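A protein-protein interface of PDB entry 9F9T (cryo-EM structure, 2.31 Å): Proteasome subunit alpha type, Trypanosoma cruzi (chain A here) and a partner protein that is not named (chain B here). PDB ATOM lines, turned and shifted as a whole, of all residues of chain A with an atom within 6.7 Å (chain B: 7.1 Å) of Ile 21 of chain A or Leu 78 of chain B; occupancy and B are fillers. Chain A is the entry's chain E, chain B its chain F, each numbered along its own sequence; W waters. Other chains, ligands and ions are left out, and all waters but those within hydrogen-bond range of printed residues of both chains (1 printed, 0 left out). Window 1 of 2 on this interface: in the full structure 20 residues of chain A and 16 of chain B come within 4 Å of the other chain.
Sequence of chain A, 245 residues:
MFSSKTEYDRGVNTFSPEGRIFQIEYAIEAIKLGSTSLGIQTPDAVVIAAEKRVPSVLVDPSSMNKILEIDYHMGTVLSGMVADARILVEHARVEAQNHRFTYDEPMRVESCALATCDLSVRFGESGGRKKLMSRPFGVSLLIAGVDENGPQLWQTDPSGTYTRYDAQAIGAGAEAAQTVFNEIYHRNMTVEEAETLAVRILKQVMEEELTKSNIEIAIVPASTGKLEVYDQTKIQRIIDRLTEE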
ATOM      1  N   VAL A  12     -21.294  12.016  31.628  1.00  0.00           N
ATOM      2  CA  VAL A  12     -21.813  10.788  32.189  1.00  0.00           C
ATOM      3  C   VAL A  12     -22.581   9.972  31.148  1.00  0.00           C
ATOM      4  O   VAL A  12     -22.725   8.761  31.299  1.00  0.00           O
ATOM      5  CB  VAL A  12     -22.655  11.193  33.406  1.00  0.00           C
ATOM      6  CG1 VAL A  12     -23.903  10.342  33.601  1.00  0.00           C
ATOM      7  CG2 VAL A  12     -21.775  11.192  34.654  1.00  0.00           C
ATOM      8  N   ASN A  13     -23.074  10.671  30.117  1.00  0.00           N
ATOM      9  CA  ASN A  13     -23.894  10.153  29.034  1.00  0.00           C
ATOM     10  C   ASN A  13     -23.066   9.783  27.797  1.00  0.00           C
ATOM     11  O   ASN A  13     -23.412   8.881  27.077  1.00  0.00           O
ATOM     12  CB  ASN A  13     -24.931  11.211  28.621  1.00  0.00           C
ATOM     13  CG  ASN A  13     -26.033  11.480  29.644  1.00  0.00           C
ATOM     14  OD1 ASN A  13     -26.524  10.596  30.360  1.00  0.00           O
ATOM     15  ND2 ASN A  13     -26.533  12.704  29.635  1.00  0.00           N
ATOM     16  N   THR A  14     -21.949  10.436  27.541  1.00  0.00           N
ATOM     17  CA  THR A  14     -21.151  10.157  26.358  1.00  0.00           C
ATOM     18  C   THR A  14     -21.061   8.679  25.943  1.00  0.00           C
ATOM     19  O   THR A  14     -20.802   7.803  26.773  1.00  0.00           O
ATOM     20  CB  THR A  14     -19.710  10.654  26.549  1.00  0.00           C
ATOM     21  OG1 THR A  14     -19.703  11.987  27.034  1.00  0.00           O
ATOM     22  CG2 THR A  14     -18.951  10.639  25.252  1.00  0.00           C
ATOM     23  N   PHE A  15     -21.218   8.476  24.620  1.00  0.00           N
ATOM     24  CA  PHE A  15     -21.000   7.248  23.881  1.00  0.00           C
ATOM     25  C   PHE A  15     -19.586   7.256  23.343  1.00  0.00           C
ATOM     26  O   PHE A  15     -19.131   8.312  22.947  1.00  0.00           O
ATOM     27  CB  PHE A  15     -21.889   7.104  22.616  1.00  0.00           C
ATOM     28  CG  PHE A  15     -23.239   6.484  22.865  1.00  0.00           C
ATOM     29  CD1 PHE A  15     -23.398   5.109  22.840  1.00  0.00           C
ATOM     30  CD2 PHE A  15     -24.309   7.266  23.262  1.00  0.00           C
ATOM     31  CE1 PHE A  15     -24.605   4.539  23.200  1.00  0.00           C
ATOM     32  CE2 PHE A  15     -25.517   6.700  23.642  1.00  0.00           C
ATOM     33  CZ  PHE A  15     -25.669   5.333  23.606  1.00  0.00           C
ATOM     34  N   SER A  16     -18.965   6.050  23.302  1.00  0.00           N
ATOM     35  CA  SER A  16     -17.680   5.769  22.661  1.00  0.00           C
ATOM     36  C   SER A  16     -17.881   5.689  21.169  1.00  0.00           C
ATOM     37  O   SER A  16     -18.999   5.521  20.736  1.00  0.00           O
ATOM     38  CB  SER A  16     -17.041   4.449  23.127  1.00  0.00           C
ATOM     39  OG  SER A  16     -17.895   3.324  22.898  1.00  0.00           O
ATOM     40  N   GLY A  19     -19.994   2.668  20.329  1.00  0.00           N
ATOM     41  CA  GLY A  19     -21.379   2.622  20.750  1.00  0.00           C
ATOM     42  C   GLY A  19     -21.511   2.091  22.165  1.00  0.00           C
ATOM     43  O   GLY A  19     -22.630   1.818  22.589  1.00  0.00           O
ATOM     44  N   ARG A  20     -20.393   2.029  22.911  1.00  0.00           N
ATOM     45  CA  ARG A  20     -20.524   1.805  24.345  1.00  0.00           C
ATOM     46  C   ARG A  20     -20.577   3.120  25.122  1.00  0.00           C
ATOM     47  O   ARG A  20     -20.042   4.140  24.724  1.00  0.00           O
ATOM     48  CB  ARG A  20     -19.448   0.842  24.803  1.00  0.00           C
ATOM     49  CG  ARG A  20     -19.634  -0.575  24.278  1.00  0.00           C
ATOM     50  CD  ARG A  20     -18.366  -1.388  24.488  1.00  0.00           C
ATOM     51  NE  ARG A  20     -18.272  -2.575  23.641  1.00  0.00           N
ATOM     52  CZ  ARG A  20     -17.300  -2.806  22.754  1.00  0.00           C
ATOM     53  NH1 ARG A  20     -16.380  -1.888  22.490  1.00  0.00           N
ATOM     54  NH2 ARG A  20     -17.265  -3.969  22.127  1.00  0.00           N
ATOM     55  N   ILE A  21     -21.316   3.108  26.210  1.00  0.00           N
ATOM     56  CA  ILE A  21     -21.356   4.208  27.159  1.00  0.00           C
ATOM     57  C   ILE A  21     -20.202   4.043  28.155  1.00  0.00           C
ATOM     58  O   ILE A  21     -20.127   3.035  28.865  1.00  0.00           O
ATOM     59  CB  ILE A  21     -22.731   4.178  27.849  1.00  0.00           C
ATOM     60  CG1 ILE A  21     -23.840   4.362  26.807  1.00  0.00           C
ATOM     61  CG2 ILE A  21     -22.828   5.208  28.982  1.00  0.00           C
ATOM     62  CD1 ILE A  21     -25.248   4.384  27.396  1.00  0.00           C
ATOM     63  N   PHE A  22     -19.344   5.062  28.258  1.00  0.00           N
ATOM     64  CA  PHE A  22     -18.112   4.931  29.020  1.00  0.00           C
ATOM     65  C   PHE A  22     -18.419   4.590  30.478  1.00  0.00           C
ATOM     66  O   PHE A  22     -17.880   3.630  31.019  1.00  0.00           O
ATOM     67  CB  PHE A  22     -17.274   6.201  28.859  1.00  0.00           C
ATOM     68  CG  PHE A  22     -16.505   6.308  27.566  1.00  0.00           C
ATOM     69  CD1 PHE A  22     -15.549   5.382  27.236  1.00  0.00           C
ATOM     70  CD2 PHE A  22     -16.767   7.327  26.661  1.00  0.00           C
ATOM     71  CE1 PHE A  22     -14.840   5.479  26.048  1.00  0.00           C
ATOM     72  CE2 PHE A  22     -16.049   7.444  25.474  1.00  0.00           C
ATOM     73  CZ  PHE A  22     -15.088   6.520  25.167  1.00  0.00           C
ATOM     74  N   GLN A  23     -19.331   5.350  31.094  1.00  0.00           N
ATOM     75  CA  GLN A  23     -19.623   5.085  32.488  1.00  0.00           C
ATOM     76  C   GLN A  23     -19.900   3.596  32.720  1.00  0.00           C
ATOM     77  O   GLN A  23     -19.474   3.070  33.748  1.00  0.00           O
ATOM     78  CB  GLN A  23     -20.738   5.988  33.054  1.00  0.00           C
ATOM     79  CG  GLN A  23     -20.281   7.420  33.402  1.00  0.00           C
ATOM     80  CD  GLN A  23     -19.203   7.407  34.468  1.00  0.00           C
ATOM     81  OE1 GLN A  23     -19.455   7.008  35.605  1.00  0.00           O
ATOM     82  NE2 GLN A  23     -17.978   7.732  34.083  1.00  0.00           N
ATOM     83  N   ILE A  24     -20.578   2.909  31.771  1.00  0.00           N
ATOM     84  CA  ILE A  24     -20.967   1.512  31.968  1.00  0.00           C
ATOM     85  C   ILE A  24     -19.796   0.556  31.741  1.00  0.00           C
ATOM     86  O   ILE A  24     -19.629  -0.399  32.509  1.00  0.00           O
ATOM     87  CB  ILE A  24     -22.215   1.135  31.150  1.00  0.00           C
ATOM     88  CG1 ILE A  24     -23.464   1.757  31.781  1.00  0.00           C
ATOM     89  CG2 ILE A  24     -22.393  -0.373  31.007  1.00  0.00           C
ATOM     90  CD1 ILE A  24     -24.618   1.935  30.802  1.00  0.00           C
ATOM     91  N   GLU A  25     -18.949   0.821  30.759  1.00  0.00           N
ATOM     92  CA  GLU A  25     -17.761   0.005  30.623  1.00  0.00           C
ATOM     93  C   GLU A  25     -16.950   0.034  31.914  1.00  0.00           C
ATOM     94  O   GLU A  25     -16.573  -1.016  32.445  1.00  0.00           O
ATOM     95  CB  GLU A  25     -16.991   0.438  29.382  1.00  0.00           C
ATOM     96  CG  GLU A  25     -17.755   0.056  28.119  1.00  0.00           C
ATOM     97  CD  GLU A  25     -18.399  -1.335  28.170  1.00  0.00           C
ATOM     98  OE1 GLU A  25     -17.640  -2.339  28.237  1.00  0.00           O
ATOM     99  OE2 GLU A  25     -19.667  -1.429  28.180  1.00  0.00           O
ATOM    100  N   TYR A  26     -16.700   1.240  32.438  1.00  0.00           N
ATOM    101  CA  TYR A  26     -15.819   1.366  33.589  1.00  0.00           C
ATOM    102  C   TYR A  26     -16.460   0.686  34.787  1.00  0.00           C
ATOM    103  O   TYR A  26     -15.764   0.080  35.569  1.00  0.00           O
ATOM    104  CB  TYR A  26     -15.459   2.817  33.930  1.00  0.00           C
ATOM    105  CG  TYR A  26     -14.843   3.668  32.816  1.00  0.00           C
ATOM    106  CD1 TYR A  26     -13.954   3.142  31.870  1.00  0.00           C
ATOM    107  CD2 TYR A  26     -15.199   5.029  32.703  1.00  0.00           C
ATOM    108  CE1 TYR A  26     -13.460   3.943  30.833  1.00  0.00           C
ATOM    109  CE2 TYR A  26     -14.698   5.829  31.693  1.00  0.00           C
ATOM    110  CZ  TYR A  26     -13.842   5.285  30.743  1.00  0.00           C
ATOM    111  OH  TYR A  26     -13.373   6.183  29.811  1.00  0.00           O
ATOM    112  N   PHE A 123     -29.593   6.821  35.673  1.00  0.00           N
ATOM    113  CA  PHE A 123     -28.494   7.748  35.956  1.00  0.00           C
ATOM    114  C   PHE A 123     -28.331   8.748  34.807  1.00  0.00           C
ATOM    115  O   PHE A 123     -28.622   8.401  33.669  1.00  0.00           O
ATOM    116  CB  PHE A 123     -27.188   6.972  36.248  1.00  0.00           C
ATOM    117  CG  PHE A 123     -26.484   6.317  35.069  1.00  0.00           C
ATOM    118  CD1 PHE A 123     -25.414   6.950  34.429  1.00  0.00           C
ATOM    119  CD2 PHE A 123     -26.850   5.049  34.621  1.00  0.00           C
ATOM    120  CE1 PHE A 123     -24.764   6.354  33.359  1.00  0.00           C
ATOM    121  CE2 PHE A 123     -26.213   4.463  33.530  1.00  0.00           C
ATOM    122  CZ  PHE A 123     -25.169   5.111  32.917  1.00  0.00           C
ATOM    123  N   SER A 159     -25.099  -2.546  32.983  1.00  0.00           N
ATOM    124  CA  SER A 159     -25.803  -2.143  31.768  1.00  0.00           C
ATOM    125  C   SER A 159     -27.303  -2.220  31.956  1.00  0.00           C
ATOM    126  O   SER A 159     -28.036  -1.606  31.204  1.00  0.00           O
ATOM    127  CB  SER A 159     -25.430  -2.959  30.549  1.00  0.00           C
ATOM    128  OG  SER A 159     -25.288  -4.325  30.854  1.00  0.00           O
ATOM    129  N   ALA B  25     -23.931   6.609  18.815  1.00  0.00           N
ATOM    130  CA  ALA B  25     -25.092   5.868  19.327  1.00  0.00           C
ATOM    131  C   ALA B  25     -25.571   4.878  18.276  1.00  0.00           C
ATOM    132  O   ALA B  25     -25.802   3.726  18.583  1.00  0.00           O
ATOM    133  CB  ALA B  25     -26.188   6.799  19.743  1.00  0.00           C
ATOM    134  N   ALA B  28     -24.075   1.560  18.296  1.00  0.00           N
ATOM    135  CA  ALA B  28     -24.551   0.575  19.262  1.00  0.00           C
ATOM    136  C   ALA B  28     -25.469  -0.451  18.595  1.00  0.00           C
ATOM    137  O   ALA B  28     -25.592  -1.589  19.070  1.00  0.00           O
ATOM    138  CB  ALA B  28     -25.314   1.186  20.430  1.00  0.00           C
ATOM    139  N   VAL B  29     -26.190   0.001  17.575  1.00  0.00           N
ATOM    140  CA  VAL B  29     -27.102  -0.831  16.808  1.00  0.00           C
ATOM    141  C   VAL B  29     -26.348  -1.751  15.851  1.00  0.00           C
ATOM    142  O   VAL B  29     -26.740  -2.890  15.663  1.00  0.00           O
ATOM    143  CB  VAL B  29     -28.076   0.051  16.021  1.00  0.00           C
ATOM    144  CG1 VAL B  29     -28.791  -0.763  14.956  1.00  0.00           C
ATOM    145  CG2 VAL B  29     -29.046   0.756  16.962  1.00  0.00           C
ATOM    146  N   GLY B  32     -25.236  -4.951  17.824  1.00  0.00           N
ATOM    147  CA  GLY B  32     -26.150  -5.916  18.424  1.00  0.00           C
ATOM    148  C   GLY B  32     -26.373  -7.082  17.465  1.00  0.00           C
ATOM    149  O   GLY B  32     -25.936  -7.033  16.314  1.00  0.00           O
ATOM    150  N   ILE B  75     -35.497  -5.624  18.942  1.00  0.00           N
ATOM    151  CA  ILE B  75     -34.442  -4.662  19.196  1.00  0.00           C
ATOM    152  C   ILE B  75     -33.057  -5.143  18.748  1.00  0.00           C
ATOM    153  O   ILE B  75     -32.870  -6.310  18.421  1.00  0.00           O
ATOM    154  CB  ILE B  75     -34.402  -4.277  20.657  1.00  0.00           C
ATOM    155  CG1 ILE B  75     -33.861  -5.410  21.549  1.00  0.00           C
ATOM    156  CG2 ILE B  75     -35.780  -3.793  21.100  1.00  0.00           C
ATOM    157  CD1 ILE B  75     -34.076  -5.196  23.081  1.00  0.00           C
ATOM    158  N   ALA B  76     -32.182  -4.150  18.561  1.00  0.00           N
ATOM    159  CA  ALA B  76     -30.742  -4.294  18.468  1.00  0.00           C
ATOM    160  C   ALA B  76     -30.026  -3.145  19.204  1.00  0.00           C
ATOM    161  O   ALA B  76     -30.375  -1.977  19.023  1.00  0.00           O
ATOM    162  CB  ALA B  76     -30.305  -4.382  17.043  1.00  0.00           C
ATOM    163  N   GLY B  77     -29.077  -3.528  20.094  1.00  0.00           N
ATOM    164  CA  GLY B  77     -28.213  -2.625  20.826  1.00  0.00           C
ATOM    165  C   GLY B  77     -28.502  -2.707  22.309  1.00  0.00           C
ATOM    166  O   GLY B  77     -28.678  -3.788  22.837  1.00  0.00           O
ATOM    167  N   LEU B  78     -28.570  -1.557  22.974  1.00  0.00           N
ATOM    168  CA  LEU B  78     -28.659  -1.507  24.422  1.00  0.00           C
ATOM    169  C   LEU B  78     -30.075  -1.846  24.829  1.00  0.00           C
ATOM    170  O   LEU B  78     -31.026  -1.163  24.483  1.00  0.00           O
ATOM    171  CB  LEU B  78     -28.255  -0.137  24.986  1.00  0.00           C
ATOM    172  CG  LEU B  78     -26.988   0.455  24.357  1.00  0.00           C
ATOM    173  CD1 LEU B  78     -26.596   1.750  25.054  1.00  0.00           C
ATOM    174  CD2 LEU B  78     -25.828  -0.551  24.319  1.00  0.00           C
ATOM    175  N   VAL B  79     -30.158  -2.923  25.585  1.00  0.00           N
ATOM    176  CA  VAL B  79     -31.409  -3.518  25.932  1.00  0.00           C
ATOM    177  C   VAL B  79     -32.130  -2.640  26.939  1.00  0.00           C
ATOM    178  O   VAL B  79     -33.361  -2.614  26.981  1.00  0.00           O
ATOM    179  CB  VAL B  79     -31.138  -4.946  26.432  1.00  0.00           C
ATOM    180  CG1 VAL B  79     -32.370  -5.598  27.020  1.00  0.00           C
ATOM    181  CG2 VAL B  79     -30.556  -5.783  25.287  1.00  0.00           C
ATOM    182  N   ALA B  80     -31.401  -1.928  27.782  1.00  0.00           N
ATOM    183  CA  ALA B  80     -32.106  -1.162  28.801  1.00  0.00           C
ATOM    184  C   ALA B  80     -32.826  -0.024  28.112  1.00  0.00           C
ATOM    185  O   ALA B  80     -33.858   0.437  28.569  1.00  0.00           O
ATOM    186  CB  ALA B  80     -31.152  -0.633  29.848  1.00  0.00           C
ATOM    187  N   ASP B  81     -32.280   0.401  26.972  1.00  0.00           N
ATOM    188  CA  ASP B  81     -32.989   1.348  26.131  1.00  0.00           C
ATOM    189  C   ASP B  81     -34.221   0.741  25.461  1.00  0.00           C
ATOM    190  O   ASP B  81     -35.286   1.355  25.522  1.00  0.00           O
ATOM    191  CB  ASP B  81     -32.020   2.005  25.189  1.00  0.00           C
ATOM    192  CG  ASP B  81     -31.141   3.013  25.917  1.00  0.00           C
ATOM    193  OD1 ASP B  81     -30.996   2.860  27.179  1.00  0.00           O
ATOM    194  OD2 ASP B  81     -30.642   3.984  25.208  1.00  0.00           O
ATOM    195  N   GLY B  82     -34.089  -0.441  24.858  1.00  0.00           N
ATOM    196  CA  GLY B  82     -35.232  -1.186  24.360  1.00  0.00           C
ATOM    197  C   GLY B  82     -36.348  -1.274  25.404  1.00  0.00           C
ATOM    198  O   GLY B  82     -37.514  -1.081  25.092  1.00  0.00           O
ATOM    199  N   ARG B  83     -36.021  -1.532  26.657  1.00  0.00           N
ATOM    200  CA  ARG B  83     -37.091  -1.771  27.603  1.00  0.00           C
ATOM    201  C   ARG B  83     -37.826  -0.480  27.906  1.00  0.00           C
ATOM    202  O   ARG B  83     -38.934  -0.508  28.441  1.00  0.00           O
ATOM    203  CB  ARG B  83     -36.613  -2.438  28.908  1.00  0.00           C
ATOM    204  CG  ARG B  83     -36.234  -3.892  28.700  1.00  0.00           C
ATOM    205  CD  ARG B  83     -36.334  -4.643  30.019  1.00  0.00           C
ATOM    206  NE  ARG B  83     -35.536  -4.009  31.062  1.00  0.00           N
ATOM    207  CZ  ARG B  83     -34.225  -4.186  31.190  1.00  0.00           C
ATOM    208  NH1 ARG B  83     -33.500  -3.346  31.918  1.00  0.00           N
ATOM    209  NH2 ARG B  83     -33.643  -5.169  30.519  1.00  0.00           N
ATOM    210  N   ARG B 127     -29.582  11.686  26.940  1.00  0.00           N
ATOM    211  CA  ARG B 127     -28.602  10.850  26.237  1.00  0.00           C
ATOM    212  C   ARG B 127     -29.320  10.296  24.990  1.00  0.00           C
ATOM    213  O   ARG B 127     -30.499   9.982  25.082  1.00  0.00           O
ATOM    214  CB  ARG B 127     -28.185   9.728  27.224  1.00  0.00           C
ATOM    215  CG  ARG B 127     -27.378   8.576  26.642  1.00  0.00           C
ATOM    216  CD  ARG B 127     -26.855   7.583  27.666  1.00  0.00           C
ATOM    217  NE  ARG B 127     -27.836   6.935  28.512  1.00  0.00           N
ATOM    218  CZ  ARG B 127     -28.633   5.937  28.117  1.00  0.00           C
ATOM    219  NH1 ARG B 127     -28.720   5.591  26.839  1.00  0.00           N
ATOM    220  NH2 ARG B 127     -29.386   5.318  29.010  1.00  0.00           N
ATOM    221  N   PRO B 128     -28.645  10.029  23.869  1.00  0.00           N
ATOM    222  CA  PRO B 128     -29.260   9.276  22.798  1.00  0.00           C
ATOM    223  C   PRO B 128     -29.721   7.924  23.295  1.00  0.00           C
ATOM    224  O   PRO B 128     -29.347   7.493  24.390  1.00  0.00           O
ATOM    225  CB  PRO B 128     -28.172   9.201  21.742  1.00  0.00           C
ATOM    226  CG  PRO B 128     -27.328  10.410  22.023  1.00  0.00           C
ATOM    227  CD  PRO B 128     -27.325  10.516  23.537  1.00  0.00           C
ATOM    228  N   PHE B 129     -30.625   7.304  22.544  1.00  0.00           N
ATOM    229  CA  PHE B 129     -31.004   5.911  22.712  1.00  0.00           C
ATOM    230  C   PHE B 129     -30.116   5.073  21.808  1.00  0.00           C
ATOM    231  O   PHE B 129     -30.023   5.350  20.620  1.00  0.00           O
ATOM    232  CB  PHE B 129     -32.437   5.675  22.254  1.00  0.00           C
ATOM    233  CG  PHE B 129     -33.474   6.260  23.171  1.00  0.00           C
ATOM    234  CD1 PHE B 129     -33.710   5.707  24.404  1.00  0.00           C
ATOM    235  CD2 PHE B 129     -34.216   7.359  22.779  1.00  0.00           C
ATOM    236  CE1 PHE B 129     -34.616   6.292  25.280  1.00  0.00           C
ATOM    237  CE2 PHE B 129     -35.163   7.914  23.634  1.00  0.00           C
ATOM    238  CZ  PHE B 129     -35.365   7.379  24.889  1.00  0.00           C
ATOM    239  N   GLY B 130     -29.463   4.043  22.361  1.00  0.00           N
ATOM    240  CA  GLY B 130     -28.511   3.296  21.570  1.00  0.00           C
ATOM    241  C   GLY B 130     -29.097   1.998  21.062  1.00  0.00           C
ATOM    242  O   GLY B 130     -28.402   1.001  21.017  1.00  0.00           O
ATOM    243  N   VAL B 131     -30.330   2.034  20.581  1.00  0.00           N
ATOM    244  CA  VAL B 131     -31.105   0.843  20.283  1.00  0.00           C
ATOM    245  C   VAL B 131     -31.935   1.111  19.031  1.00  0.00           C
ATOM    246  O   VAL B 131     -32.434   2.197  18.826  1.00  0.00           O
ATOM    247  CB  VAL B 131     -31.976   0.537  21.502  1.00  0.00           C
ATOM    248  CG1 VAL B 131     -33.122   1.520  21.637  1.00  0.00           C
ATOM    249  CG2 VAL B 131     -32.505  -0.896  21.501  1.00  0.00           C
ATOM    250  N   GLY B 132     -31.935   0.162  18.136  1.00  0.00           N
ATOM    251  CA  GLY B 132     -32.728   0.203  16.936  1.00  0.00           C
ATOM    252  C   GLY B 132     -33.968  -0.669  17.132  1.00  0.00           C
ATOM    253  O   GLY B 132     -33.935  -1.571  17.951  1.00  0.00           O
HETATM  254  O   HOH W   1     -28.402  -2.305  28.177  1.00  0.00           O
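Among the printed residues, pairs that only touch across the chains: Gly 19 of chain A with Ala 28 of chain B (3.5 Å), Ser 159 of chain A with Ala 80 of chain B (3.5 Å), Ile 21 of chain A with Arg 127 of chain B (3.6 Å), Asn 13 of chain A with Arg 127 of chain B (3.7 Å), Ile 21 of chain A with Leu 78 of chain B (3.8 Å), Phe 15 of chain A with Leu 78 of chain B (3.9 Å), Phe 15 of chain A with Ala 25 of chain B (3.96 Å), Phe 15 of chain A with Pro 128 of chain B (3.98 Å) and Phe 15 of chain A with Arg 127 of chain B (3.998 Å).
Of the printed residues of chain B, Asn 13 of chain A touches Arg 127. Of the printed residues of chain B, Phe 15 of chain A touches Ala 25 (3.96 Å), Leu 78 (3.9 Å), Arg 127 (3.998 Å) and Pro 128 (3.98 Å). Of the printed residues of chain A, Leu 78 of chain B touches Phe 15 (3.9 Å) and Ile 21 (3.8 Å). The nearest residue of chain B that does not touch Ile 21 of chain A is Asp 81 of chain B (5.8 Å). The nearest residue of chain A that does not touch Leu 78 of chain B is Gly 19 of chain A (4.3 Å).
Water W1 lies within hydrogen-bond range of the backbone NH of Ala 80 of chain B, the backbone carbonyl oxygen of Ser 159 of chain A and the backbone NH of Val 79 of chain B.
Hydrophobic or aromatic side chains of chain A that line the printed part of chain B: Phe 15 and Ile 21. Of the 19 printed residues of chain B, 6 touch a printed residue of chain A. Hydrophobic or aromatic side chains of chain B within 4 Å of the printed part of chain A: Ala 25, Ala 28, Leu 78 and Ala 80. Among the printed residues, 9 pairs touch across the chains.
OG of Ser 16 of chain A is in hydrogen-bond range of N of Gly 19 of chain A. The backbone NH (N) of Leu 78 of chain B is in hydrogen-bond range of the backbone carbonyl oxygen (O) of Gly 130 of chain B (3.2 Å). OD2 of Asp 81 of chain B is in salt-bridge range of NH1 of Arg 127 of chain B (3.0 Å).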
